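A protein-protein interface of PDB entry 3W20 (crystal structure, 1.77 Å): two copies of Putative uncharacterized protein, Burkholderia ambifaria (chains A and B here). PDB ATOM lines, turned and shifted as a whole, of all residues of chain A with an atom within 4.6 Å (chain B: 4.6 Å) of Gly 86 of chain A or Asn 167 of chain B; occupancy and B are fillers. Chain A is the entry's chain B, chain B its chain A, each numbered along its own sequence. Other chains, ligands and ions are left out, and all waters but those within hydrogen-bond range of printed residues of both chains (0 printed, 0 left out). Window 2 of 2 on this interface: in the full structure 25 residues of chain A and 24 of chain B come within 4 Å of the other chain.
Of the 9 printed residues of chain A, 4 touch a printed residue of chain B.
Printed residues of chain A that touch a printed residue of chain B: Gly 86, Asp 87, Val 90 and Asn 167.
Printed residues of chain B that touch a printed residue of chain A: Gly 86, Leu 89, Val 166, Asn 167, Trp 168 and Pro 169.
Hydrophobic or aromatic side chains of chain B within 4 Å of the printed part of chain A: Leu 89 and Pro 169.
Among the printed residues, no Asp or Glu carboxylate lies within 4 Å of a Lys or Arg side-chain nitrogen of the other chain.
Asn 167 of chain B touches Gly 86 of chain A (OD1 to CA, 3.1 Å).
Val 166 of chain B touches Asp 87 of chain A.
Asn 167 of chain B touches Asp 87 of chain A.
O of Trp 168 of chain B touches CB of Asp 87 of chain A, 3.8 Å away.
Pro 169 of chain B touches Asp 87 of chain A (CB to O, 3.7 Å).
Val 90 of chain A touches Leu 89 of chain B (CG2 to CD2, 3.8 Å).
Val 90 of chain A touches Asn 167 of chain B (CG2 to O, 3.3 Å).
Pro 169 of chain B touches Val 90 of chain A.
OD1 of Asn 167 of chain A touches CA of Gly 86 of chain B, at 3.0 Å.
Asn 167 of chain B touches Asn 167 of chain A.
N of Gly 86 of chain B lies within hydrogen-bond range of OD2 of Asp 164 of chain B.
The backbone NH of Val 166 of chain B sits close to the side-chain carboxylate of Asp 164 of chain B.
The side-chain amide nitrogen (ND2) of Asn 167 of chain B sits at hydrogen-bond distance from the side-chain carboxylate (OD2) of Asp 164 of chain B, 2.9 Å away.
OD2 of Asp 164 of chain A is in hydrogen-bond range of N of Gly 86 of chain A, at 2.7 Å.
ND2 of Asn 167 of chain A is in hydrogen-bond range of OD2 of Asp 164 of chain A, 2.9 Å away.
Gly 86 of chain A touches Asn 167 of chain B, and with the chains exchanged Asn 167 of chain A touches Gly 86 of chain B.
Asn 167 of chain B touches its own counterpart, Asn 167 of chain A.
Positions printed for both chains: 86, 89, 164 and 167.
Of the 10 pairs that touch across the chains among the printed residues, 3 have their exchanged pair printed and touching as well.
Of chain B, only Asn 167 (3.1 Å) comes within 4 Å of Gly 86 of chain A.
Asp 164 of chain A touches none of the printed residues of chain B.
Of the printed residues of chain B, Asn 167 of chain A touches Gly 86 (3.0 Å) and Asn 167 (3.5 Å).
Of the printed residues of chain A, Gly 86 of chain B touches Asn 167.
Of the printed residues of chain A, Leu 89 of chain B touches Val 90.
Of chain A, only Gly 86, Asp 87, Val 90 and Asn 167 come within 4 Å of Asn 167 of chain B.
Printed residues of chain A within 4 Å of Trp 168 of chain B: Asp 87.
Printed residues of chain A within 4 Å of Pro 169 of chain B: Asp 87 and Val 90.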
ATOM      1  N   GLU A  84       1.682 -15.139  19.841  1.00  0.00           N
ATOM      2  CA  GLU A  84       2.403 -13.964  19.347  1.00  0.00           C
ATOM      3  C   GLU A  84       2.161 -13.708  17.836  1.00  0.00           C
ATOM      4  O   GLU A  84       1.930 -14.615  17.050  1.00  0.00           O
ATOM      5  CB  GLU A  84       3.895 -14.082  19.631  1.00  0.00           C
ATOM      6  CG  GLU A  84       4.193 -14.302  21.092  1.00  0.00           C
ATOM      7  CD  GLU A  84       3.963 -13.057  21.943  1.00  0.00           C
ATOM      8  OE1 GLU A  84       3.811 -11.936  21.432  1.00  0.00           O
ATOM      9  OE2 GLU A  84       3.840 -13.238  23.139  1.00  0.00           O
ATOM     10  N   GLN A  85       2.326 -12.451  17.422  1.00  0.00           N
ATOM     11  CA  GLN A  85       2.024 -12.062  16.051  1.00  0.00           C
ATOM     12  C   GLN A  85       3.122 -11.130  15.532  1.00  0.00           C
ATOM     13  O   GLN A  85       3.735 -10.366  16.336  1.00  0.00           O
ATOM     14  CB  GLN A  85       0.639 -11.368  16.020  1.00  0.00           C
ATOM     15  CG  GLN A  85      -0.460 -12.410  16.025  1.00  0.00           C
ATOM     16  CD  GLN A  85      -1.842 -11.856  15.768  1.00  0.00           C
ATOM     17  OE1 GLN A  85      -2.434 -11.209  16.635  1.00  0.00           O
ATOM     18  NE2 GLN A  85      -2.376 -12.132  14.571  1.00  0.00           N
ATOM     19  N   GLY A  86       3.392 -11.253  14.230  1.00  0.00           N
ATOM     20  CA  GLY A  86       4.275 -10.303  13.541  1.00  0.00           C
ATOM     21  C   GLY A  86       5.689 -10.344  14.077  1.00  0.00           C
ATOM     22  O   GLY A  86       6.229 -11.383  14.309  1.00  0.00           O
ATOM     23  N   ASP A  87       6.321  -9.175  14.229  1.00  0.00           N
ATOM     24  CA  ASP A  87       7.693  -9.163  14.769  1.00  0.00           C
ATOM     25  C   ASP A  87       7.869  -9.799  16.133  1.00  0.00           C
ATOM     26  O   ASP A  87       8.933 -10.330  16.453  1.00  0.00           O
ATOM     27  CB  ASP A  87       8.421  -7.775  14.661  1.00  0.00           C
ATOM     28  CG  ASP A  87       7.689  -6.549  15.299  1.00  0.00           C
ATOM     29  OD1 ASP A  87       6.585  -6.565  15.826  1.00  0.00           O
ATOM     30  OD2 ASP A  87       8.306  -5.467  15.222  1.00  0.00           O
ATOM     31  N   LYS A  88       6.821  -9.793  16.939  1.00  0.00           N
ATOM     32  CA  LYS A  88       6.943 -10.380  18.281  1.00  0.00           C
ATOM     33  C   LYS A  88       6.996 -11.879  18.229  1.00  0.00           C
ATOM     34  O   LYS A  88       7.538 -12.513  19.154  1.00  0.00           O
ATOM     35  CB  LYS A  88       5.770  -9.977  19.157  1.00  0.00           C
ATOM     36  CG  LYS A  88       5.766  -8.498  19.540  1.00  0.00           C
ATOM     37  CD  LYS A  88       4.717  -8.302  20.642  1.00  0.00           C
ATOM     38  CE  LYS A  88       5.157  -7.274  21.680  1.00  0.00           C
ATOM     39  NZ  LYS A  88       5.129  -5.889  21.116  1.00  0.00           N
ATOM     40  N   LEU A  89       6.381 -12.430  17.174  1.00  0.00           N
ATOM     41  CA  LEU A  89       6.468 -13.877  16.885  1.00  0.00           C
ATOM     42  C   LEU A  89       7.895 -14.241  16.532  1.00  0.00           C
ATOM     43  O   LEU A  89       8.409 -15.228  17.059  1.00  0.00           O
ATOM     44  CB  LEU A  89       5.504 -14.331  15.761  1.00  0.00           C
ATOM     45  CG  LEU A  89       5.679 -15.792  15.275  1.00  0.00           C
ATOM     46  CD1 LEU A  89       5.441 -16.681  16.481  1.00  0.00           C
ATOM     47  CD2 LEU A  89       4.632 -15.926  14.165  1.00  0.00           C
ATOM     48  N   VAL A  90       8.579 -13.399  15.745  1.00  0.00           N
ATOM     49  CA  VAL A  90       9.937 -13.746  15.360  1.00  0.00           C
ATOM     50  C   VAL A  90      10.827 -13.637  16.581  1.00  0.00           C
ATOM     51  O   VAL A  90      11.627 -14.506  16.868  1.00  0.00           O
ATOM     52  CB  VAL A  90      10.464 -12.834  14.230  1.00  0.00           C
ATOM     53  CG1 VAL A  90      11.887 -13.216  13.895  1.00  0.00           C
ATOM     54  CG2 VAL A  90       9.604 -12.894  13.029  1.00  0.00           C
ATOM     55  N   ASP A 164      -1.093 -16.101  14.337  1.00  0.00           N
ATOM     56  CA  ASP A 164      -0.643 -15.425  13.144  1.00  0.00           C
ATOM     57  C   ASP A 164      -0.487 -16.435  12.006  1.00  0.00           C
ATOM     58  O   ASP A 164       0.648 -16.881  11.658  1.00  0.00           O
ATOM     59  CB  ASP A 164       0.680 -14.640  13.460  1.00  0.00           C
ATOM     60  CG  ASP A 164       1.097 -13.718  12.308  1.00  0.00           C
ATOM     61  OD1 ASP A 164       0.501 -13.805  11.210  1.00  0.00           O
ATOM     62  OD2 ASP A 164       2.079 -12.960  12.535  1.00  0.00           O
ATOM     63  N   ASN A 167       2.154 -16.316   9.152  1.00  0.00           N
ATOM     64  CA  ASN A 167       3.549 -16.386   9.585  1.00  0.00           C
ATOM     65  C   ASN A 167       3.842 -17.615  10.447  1.00  0.00           C
ATOM     66  O   ASN A 167       4.987 -17.860  10.806  1.00  0.00           O
ATOM     67  CB  ASN A 167       3.930 -15.114  10.336  1.00  0.00           C
ATOM     68  CG  ASN A 167       3.885 -13.884   9.434  1.00  0.00           C
ATOM     69  OD1 ASN A 167       4.304 -13.950   8.285  1.00  0.00           O
ATOM     70  ND2 ASN A 167       3.306 -12.819   9.920  1.00  0.00           N
ATOM     71  N   GLY B  86       8.141 -13.597   6.356  1.00  0.00           N
ATOM     72  CA  GLY B  86       6.904 -14.263   6.838  1.00  0.00           C
ATOM     73  C   GLY B  86       7.202 -15.580   7.573  1.00  0.00           C
ATOM     74  O   GLY B  86       8.075 -15.623   8.410  1.00  0.00           O
ATOM     75  N   LEU B  89      10.772 -16.595   7.661  1.00  0.00           N
ATOM     76  CA  LEU B  89      11.609 -15.846   8.584  1.00  0.00           C
ATOM     77  C   LEU B  89      11.449 -16.448   9.990  1.00  0.00           C
ATOM     78  O   LEU B  89      12.440 -16.603  10.711  1.00  0.00           O
ATOM     79  CB  LEU B  89      11.204 -14.376   8.612  1.00  0.00           C
ATOM     80  CG  LEU B  89      11.704 -13.567   9.731  1.00  0.00           C
ATOM     81  CD1 LEU B  89      13.233 -13.481   9.560  1.00  0.00           C
ATOM     82  CD2 LEU B  89      11.164 -12.133   9.617  1.00  0.00           C
ATOM     83  N   ASP B 164      11.755  -8.256   5.312  1.00  0.00           N
ATOM     84  CA  ASP B 164      10.354  -8.189   5.755  1.00  0.00           C
ATOM     85  C   ASP B 164      10.237  -7.103   6.780  1.00  0.00           C
ATOM     86  O   ASP B 164      10.488  -7.363   7.942  1.00  0.00           O
ATOM     87  CB  ASP B 164       9.958  -9.569   6.324  1.00  0.00           C
ATOM     88  CG  ASP B 164       8.488  -9.648   6.724  1.00  0.00           C
ATOM     89  OD1 ASP B 164       7.888  -8.577   7.049  1.00  0.00           O
ATOM     90  OD2 ASP B 164       7.973 -10.796   6.816  1.00  0.00           O
ATOM     91  N   THR B 165       9.858  -5.878   6.353  1.00  0.00           N
ATOM     92  CA  THR B 165       9.960  -4.724   7.236  1.00  0.00           C
ATOM     93  C   THR B 165       9.110  -4.895   8.458  1.00  0.00           C
ATOM     94  O   THR B 165       9.489  -4.486   9.578  1.00  0.00           O
ATOM     95  CB  THR B 165       9.474  -3.432   6.512  1.00  0.00           C
ATOM     96  OG1 THR B 165      10.108  -3.443   5.227  1.00  0.00           O
ATOM     97  CG2 THR B 165       9.919  -2.221   7.330  1.00  0.00           C
ATOM     98  N   VAL B 166       7.920  -5.469   8.286  1.00  0.00           N
ATOM     99  CA  VAL B 166       6.984  -5.510   9.400  1.00  0.00           C
ATOM    100  C   VAL B 166       7.407  -6.524  10.467  1.00  0.00           C
ATOM    101  O   VAL B 166       7.348  -6.238  11.666  1.00  0.00           O
ATOM    102  CB  VAL B 166       5.593  -5.898   8.883  1.00  0.00           C
ATOM    103  CG1 VAL B 166       4.623  -6.120  10.024  1.00  0.00           C
ATOM    104  CG2 VAL B 166       5.095  -4.755   8.006  1.00  0.00           C
ATOM    105  N   ASN B 167       7.822  -7.681   9.999  1.00  0.00           N
ATOM    106  CA  ASN B 167       8.118  -8.810  10.897  1.00  0.00           C
ATOM    107  C   ASN B 167       9.570  -8.903  11.353  1.00  0.00           C
ATOM    108  O   ASN B 167       9.860  -9.643  12.269  1.00  0.00           O
ATOM    109  CB  ASN B 167       7.690 -10.107  10.144  1.00  0.00           C
ATOM    110  CG  ASN B 167       6.210 -10.127   9.889  1.00  0.00           C
ATOM    111  OD1 ASN B 167       5.436  -9.737  10.754  1.00  0.00           O
ATOM    112  ND2 ASN B 167       5.798 -10.609   8.722  1.00  0.00           N
ATOM    113  N   TRP B 168      10.481  -8.136  10.740  1.00  0.00           N
ATOM    114  CA  TRP B 168      11.859  -8.086  11.248  1.00  0.00           C
ATOM    115  C   TRP B 168      11.892  -7.445  12.660  1.00  0.00           C
ATOM    116  O   TRP B 168      11.463  -6.293  12.861  1.00  0.00           O
ATOM    117  CB  TRP B 168      12.705  -7.232  10.246  1.00  0.00           C
ATOM    118  CG  TRP B 168      14.187  -7.332  10.634  1.00  0.00           C
ATOM    119  CD1 TRP B 168      15.016  -6.314  11.180  1.00  0.00           C
ATOM    120  CD2 TRP B 168      14.971  -8.541  10.693  1.00  0.00           C
ATOM    121  NE1 TRP B 168      16.254  -6.790  11.502  1.00  0.00           N
ATOM    122  CE2 TRP B 168      16.311  -8.141  11.218  1.00  0.00           C
ATOM    123  CE3 TRP B 168      14.748  -9.886  10.324  1.00  0.00           C
ATOM    124  CZ2 TRP B 168      17.338  -9.044  11.374  1.00  0.00           C
ATOM    125  CZ3 TRP B 168      15.810 -10.793  10.478  1.00  0.00           C
ATOM    126  CH2 TRP B 168      17.088 -10.389  10.997  1.00  0.00           C
ATOM    127  N   PRO B 169      12.446  -8.122  13.664  1.00  0.00           N
ATOM    128  CA  PRO B 169      12.225  -7.578  15.026  1.00  0.00           C
ATOM    129  C   PRO B 169      13.301  -6.609  15.553  1.00  0.00           C
ATOM    130  O   PRO B 169      13.108  -5.958  16.579  1.00  0.00           O
ATOM    131  CB  PRO B 169      12.242  -8.825  15.871  1.00  0.00           C
ATOM    132  CG  PRO B 169      13.302  -9.692  15.174  1.00  0.00           C
ATOM    133  CD  PRO B 169      12.853  -9.550  13.697  1.00  0.00           C
